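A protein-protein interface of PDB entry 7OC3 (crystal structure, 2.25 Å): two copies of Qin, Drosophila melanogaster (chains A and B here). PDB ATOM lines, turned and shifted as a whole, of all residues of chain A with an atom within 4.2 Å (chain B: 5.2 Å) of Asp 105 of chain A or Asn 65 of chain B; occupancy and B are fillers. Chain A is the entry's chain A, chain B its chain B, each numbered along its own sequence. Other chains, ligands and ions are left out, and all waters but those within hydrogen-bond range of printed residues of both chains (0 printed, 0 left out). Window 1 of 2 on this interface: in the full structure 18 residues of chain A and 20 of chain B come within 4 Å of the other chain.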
ATOM      1  N   ILE A  81     -23.519   0.839 -12.249  1.00  0.00           N
ATOM      2  CA  ILE A  81     -23.726   2.210 -11.807  1.00  0.00           C
ATOM      3  C   ILE A  81     -22.454   3.029 -12.013  1.00  0.00           C
ATOM      4  O   ILE A  81     -21.473   2.860 -11.281  1.00  0.00           O
ATOM      5  CB  ILE A  81     -24.145   2.260 -10.326  1.00  0.00           C
ATOM      6  CG1 ILE A  81     -25.439   1.467 -10.113  1.00  0.00           C
ATOM      7  CG2 ILE A  81     -24.318   3.695  -9.867  1.00  0.00           C
ATOM      8  CD1 ILE A  81     -25.474   0.661  -8.829  1.00  0.00           C
ATOM      9  N   THR A  86     -20.647  12.124  -5.931  1.00  0.00           N
ATOM     10  CA  THR A  86     -20.552  11.630  -4.563  1.00  0.00           C
ATOM     11  C   THR A  86     -19.647  10.401  -4.443  1.00  0.00           C
ATOM     12  O   THR A  86     -18.981  10.212  -3.427  1.00  0.00           O
ATOM     13  CB  THR A  86     -21.940  11.293  -4.008  1.00  0.00           C
ATOM     14  OG1 THR A  86     -22.592  10.378  -4.896  1.00  0.00           O
ATOM     15  CG2 THR A  86     -22.775  12.558  -3.890  1.00  0.00           C
ATOM     16  N   ARG A  91     -19.909   1.055  -9.629  1.00  0.00           N
ATOM     17  CA  ARG A  91     -20.548   0.151  -8.681  1.00  0.00           C
ATOM     18  C   ARG A  91     -21.551  -0.708  -9.426  1.00  0.00           C
ATOM     19  O   ARG A  91     -21.797  -0.483 -10.613  1.00  0.00           O
ATOM     20  CB  ARG A  91     -21.217   0.931  -7.554  1.00  0.00           C
ATOM     21  CG  ARG A  91     -20.238   1.472  -6.528  1.00  0.00           C
ATOM     22  CD  ARG A  91     -20.930   2.414  -5.567  1.00  0.00           C
ATOM     23  NE  ARG A  91     -21.705   3.417  -6.288  1.00  0.00           N
ATOM     24  CZ  ARG A  91     -22.401   4.386  -5.705  1.00  0.00           C
ATOM     25  NH1 ARG A  91     -22.425   4.483  -4.383  1.00  0.00           N
ATOM     26  NH2 ARG A  91     -23.076   5.257  -6.445  1.00  0.00           N
ATOM     27  N   TYR A  92     -22.104  -1.710  -8.752  1.00  0.00           N
ATOM     28  CA  TYR A  92     -23.042  -2.612  -9.410  1.00  0.00           C
ATOM     29  C   TYR A  92     -24.293  -2.905  -8.584  1.00  0.00           C
ATOM     30  O   TYR A  92     -24.305  -2.752  -7.361  1.00  0.00           O
ATOM     31  CB  TYR A  92     -22.333  -3.927  -9.780  1.00  0.00           C
ATOM     32  CG  TYR A  92     -21.002  -3.722 -10.477  1.00  0.00           C
ATOM     33  CD1 TYR A  92     -19.831  -3.520  -9.755  1.00  0.00           C
ATOM     34  CD2 TYR A  92     -20.927  -3.692 -11.866  1.00  0.00           C
ATOM     35  CE1 TYR A  92     -18.617  -3.313 -10.399  1.00  0.00           C
ATOM     36  CE2 TYR A  92     -19.721  -3.483 -12.516  1.00  0.00           C
ATOM     37  CZ  TYR A  92     -18.570  -3.297 -11.780  1.00  0.00           C
ATOM     38  OH  TYR A  92     -17.372  -3.094 -12.431  1.00  0.00           O
ATOM     39  N   ASP A 104     -28.088  -2.572  -4.199  1.00  0.00           N
ATOM     40  CA  ASP A 104     -27.485  -1.485  -4.969  1.00  0.00           C
ATOM     41  C   ASP A 104     -26.148  -1.078  -4.361  1.00  0.00           C
ATOM     42  O   ASP A 104     -25.844  -1.433  -3.223  1.00  0.00           O
ATOM     43  CB  ASP A 104     -28.415  -0.262  -5.030  1.00  0.00           C
ATOM     44  CG  ASP A 104     -29.659  -0.500  -5.876  1.00  0.00           C
ATOM     45  OD1 ASP A 104     -29.518  -0.844  -7.069  1.00  0.00           O
ATOM     46  OD2 ASP A 104     -30.780  -0.325  -5.352  1.00  0.00           O
ATOM     47  N   ASP A 105     -25.351  -0.344  -5.134  1.00  0.00           N
ATOM     48  CA  ASP A 105     -24.090   0.228  -4.658  1.00  0.00           C
ATOM     49  C   ASP A 105     -23.103  -0.827  -4.164  1.00  0.00           C
ATOM     50  O   ASP A 105     -22.473  -0.671  -3.114  1.00  0.00           O
ATOM     51  CB  ASP A 105     -24.354   1.242  -3.543  1.00  0.00           C
ATOM     52  CG  ASP A 105     -25.265   2.374  -3.984  1.00  0.00           C
ATOM     53  OD1 ASP A 105     -25.355   2.627  -5.206  1.00  0.00           O
ATOM     54  OD2 ASP A 105     -25.879   3.018  -3.105  1.00  0.00           O
ATOM     55  N   VAL A 106     -22.967  -1.903  -4.925  1.00  0.00           N
ATOM     56  CA  VAL A 106     -22.022  -2.940  -4.561  1.00  0.00           C
ATOM     57  C   VAL A 106     -20.682  -2.676  -5.242  1.00  0.00           C
ATOM     58  O   VAL A 106     -20.608  -2.620  -6.469  1.00  0.00           O
ATOM     59  CB  VAL A 106     -22.545  -4.326  -4.947  1.00  0.00           C
ATOM     60  CG1 VAL A 106     -21.534  -5.392  -4.569  1.00  0.00           C
ATOM     61  CG2 VAL A 106     -23.885  -4.586  -4.267  1.00  0.00           C
ATOM     62  N   HIS A 107     -19.633  -2.499  -4.441  1.00  0.00           N
ATOM     63  CA  HIS A 107     -18.281  -2.281  -4.966  1.00  0.00           C
ATOM     64  C   HIS A 107     -17.728  -3.543  -5.611  1.00  0.00           C
ATOM     65  O   HIS A 107     -18.127  -4.662  -5.275  1.00  0.00           O
ATOM     66  CB  HIS A 107     -17.322  -1.824  -3.862  1.00  0.00           C
ATOM     67  CG  HIS A 107     -17.592  -0.441  -3.348  1.00  0.00           C
ATOM     68  ND1 HIS A 107     -18.865   0.055  -3.182  1.00  0.00           N
ATOM     69  CD2 HIS A 107     -16.747   0.532  -2.941  1.00  0.00           C
ATOM     70  CE1 HIS A 107     -18.793   1.287  -2.703  1.00  0.00           C
ATOM     71  NE2 HIS A 107     -17.523   1.600  -2.548  1.00  0.00           N
ATOM     72  N   TYR B  10     -23.605  14.200  -0.323  1.00  0.00           N
ATOM     73  CA  TYR B  10     -24.606  13.183  -0.627  1.00  0.00           C
ATOM     74  C   TYR B  10     -25.864  13.813  -1.225  1.00  0.00           C
ATOM     75  O   TYR B  10     -26.317  14.861  -0.769  1.00  0.00           O
ATOM     76  CB  TYR B  10     -24.965  12.385   0.636  1.00  0.00           C
ATOM     77  CG  TYR B  10     -26.157  11.466   0.450  1.00  0.00           C
ATOM     78  CD1 TYR B  10     -26.023  10.234  -0.183  1.00  0.00           C
ATOM     79  CD2 TYR B  10     -27.426  11.853   0.870  1.00  0.00           C
ATOM     80  CE1 TYR B  10     -27.116   9.400  -0.368  1.00  0.00           C
ATOM     81  CE2 TYR B  10     -28.526  11.029   0.686  1.00  0.00           C
ATOM     82  CZ  TYR B  10     -28.365   9.806   0.070  1.00  0.00           C
ATOM     83  OH  TYR B  10     -29.459   8.991  -0.111  1.00  0.00           O
ATOM     84  N   GLN B  63     -23.215   0.368   6.336  1.00  0.00           N
ATOM     85  CA  GLN B  63     -22.523   0.585   5.079  1.00  0.00           C
ATOM     86  C   GLN B  63     -23.213   1.722   4.339  1.00  0.00           C
ATOM     87  O   GLN B  63     -24.306   1.554   3.794  1.00  0.00           O
ATOM     88  CB  GLN B  63     -22.500  -0.691   4.231  1.00  0.00           C
ATOM     89  CG  GLN B  63     -21.724  -0.556   2.930  1.00  0.00           C
ATOM     90  CD  GLN B  63     -21.506  -1.883   2.226  1.00  0.00           C
ATOM     91  OE1 GLN B  63     -21.752  -2.950   2.793  1.00  0.00           O
ATOM     92  NE2 GLN B  63     -21.040  -1.823   0.982  1.00  0.00           N
ATOM     93  N   ALA B  64     -22.570   2.883   4.324  1.00  0.00           N
ATOM     94  CA  ALA B  64     -23.146   4.045   3.666  1.00  0.00           C
ATOM     95  C   ALA B  64     -22.902   3.963   2.170  1.00  0.00           C
ATOM     96  O   ALA B  64     -22.285   3.012   1.676  1.00  0.00           O
ATOM     97  CB  ALA B  64     -22.579   5.335   4.233  1.00  0.00           C
ATOM     98  N   ASN B  65     -23.382   4.980   1.469  1.00  0.00           N
ATOM     99  CA  ASN B  65     -23.431   4.997   0.015  1.00  0.00           C
ATOM    100  C   ASN B  65     -22.138   4.570  -0.690  1.00  0.00           C
ATOM    101  O   ASN B  65     -22.150   3.634  -1.493  1.00  0.00           O
ATOM    102  CB  ASN B  65     -23.833   6.403  -0.442  1.00  0.00           C
ATOM    103  CG  ASN B  65     -23.435   6.688  -1.871  1.00  0.00           C
ATOM    104  OD1 ASN B  65     -23.709   5.896  -2.773  1.00  0.00           O
ATOM    105  ND2 ASN B  65     -22.795   7.834  -2.091  1.00  0.00           N
ATOM    106  N   CYS B  66     -21.021   5.214  -0.372  1.00  0.00           N
ATOM    107  CA  CYS B  66     -19.779   4.915  -1.083  1.00  0.00           C
ATOM    108  C   CYS B  66     -18.824   4.072  -0.243  1.00  0.00           C
ATOM    109  O   CYS B  66     -17.613   4.070  -0.474  1.00  0.00           O
ATOM    110  CB  CYS B  66     -19.089   6.205  -1.530  1.00  0.00           C
ATOM    111  SG  CYS B  66     -18.099   6.018  -3.047  1.00  0.00           S
ATOM    112  N   ASP B  67     -19.377   3.353   0.726  1.00  0.00           N
ATOM    113  CA  ASP B  67     -18.584   2.484   1.587  1.00  0.00           C
ATOM    114  C   ASP B  67     -18.556   1.059   1.040  1.00  0.00           C
ATOM    115  O   ASP B  67     -19.601   0.497   0.712  1.00  0.00           O
ATOM    116  CB  ASP B  67     -19.146   2.478   3.010  1.00  0.00           C
ATOM    117  CG  ASP B  67     -19.055   3.831   3.683  1.00  0.00           C
ATOM    118  OD1 ASP B  67     -18.331   4.712   3.173  1.00  0.00           O
ATOM    119  OD2 ASP B  67     -19.707   4.010   4.732  1.00  0.00           O
ATOM    120  N   LEU B  99     -23.066  12.739   6.877  1.00  0.00           N
ATOM    121  CA  LEU B  99     -23.211  12.417   5.458  1.00  0.00           C
ATOM    122  C   LEU B  99     -24.520  12.962   4.889  1.00  0.00           C
ATOM    123  O   LEU B  99     -24.543  13.537   3.801  1.00  0.00           O
ATOM    124  CB  LEU B  99     -23.145  10.904   5.246  1.00  0.00           C
ATOM    125  CG  LEU B  99     -22.769  10.391   3.856  1.00  0.00           C
ATOM    126  CD1 LEU B  99     -21.732  11.288   3.203  1.00  0.00           C
ATOM    127  CD2 LEU B  99     -22.277   8.954   3.929  1.00  0.00           C
ATOM    128  N   GLU B 101     -27.329  10.906   4.606  1.00  0.00           N
ATOM    129  CA  GLU B 101     -28.066   9.820   3.971  1.00  0.00           C
ATOM    130  C   GLU B 101     -28.923   9.059   4.977  1.00  0.00           C
ATOM    131  O   GLU B 101     -28.525   8.879   6.127  1.00  0.00           O
ATOM    132  CB  GLU B 101     -27.097   8.862   3.268  1.00  0.00           C
ATOM    133  CG  GLU B 101     -27.713   7.541   2.813  1.00  0.00           C
ATOM    134  CD  GLU B 101     -26.672   6.556   2.315  1.00  0.00           C
ATOM    135  OE1 GLU B 101     -25.469   6.865   2.424  1.00  0.00           O
ATOM    136  OE2 GLU B 101     -27.053   5.474   1.818  1.00  0.00           O
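Along chain A the printed residues that touch a printed residue of chain B span positions 86 to 107.
Among the printed residues, 6 pairs touch across the chains.
Among the printed residues, merely in contact across the chains: His 107 of chain A with Asp 67 of chain B, Asp 105 of chain A with Asn 65 of chain B, Thr 86 of chain A with Asn 65 of chain B and Thr 86 of chain A with Tyr 10 of chain B.
O of Cys 66 of chain B lies within hydrogen-bond range of NE2 of His 107 of chain A, at 3.2 Å.
The guanidinium group (NH1) of Arg 91 of chain A lies within hydrogen-bond range of the side-chain amide oxygen (OD1) of Asn 65 of chain B (2.5 Å).
Of chain B, only Asn 65 (3.6 Å) comes within 4 Å of Asp 105 of chain A.
Printed residues of chain B within 4 Å of His 107 of chain A: Cys 66 (3.2 Å) and Asp 67 (3.6 Å).
Ala 64 of chain B touches none of the printed residues of chain A.
Asn 65 of chain B touches three residues of chain A.
Printed residues of chain A within 4 Å of Cys 66 of chain B: His 107 (3.2 Å).
The nearest residue of chain B that does not touch Asp 105 of chain A is Gln 63 of chain B (4.5 Å).
The nearest printed residue of chain B that does not touch Thr 86 of chain A is Cys 66 of chain B (4.3 Å).
OE1 of Glu 101 of chain B sits at hydrogen-bond distance from N of Asn 65 of chain B, 3.0 Å away.
The backbone carbonyl oxygen (O) of Arg 91 of chain A sits at hydrogen-bond distance from the backbone NH (N) of Ile 81 of chain A (2.7 Å).
NE2 of Gln 63 of chain B lies within hydrogen-bond range of O of Asp 67 of chain B, 2.7 Å away.
N of Asp 105 of chain A is in hydrogen-bond range of O of Tyr 92 of chain A (3.4 Å).
The backbone NH of Ala 64 of chain B sits at hydrogen-bond distance from the side-chain carboxylate of Asp 67 of chain B.
NH1 of Arg 91 of chain A is in salt-bridge range of OD1 of Asp 105 of chain A (3.6 Å).
No position is printed for both chains.
Of the 6 pairs that touch across the chains among the printed residues, none has its exchanged pair printed and touching as well.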
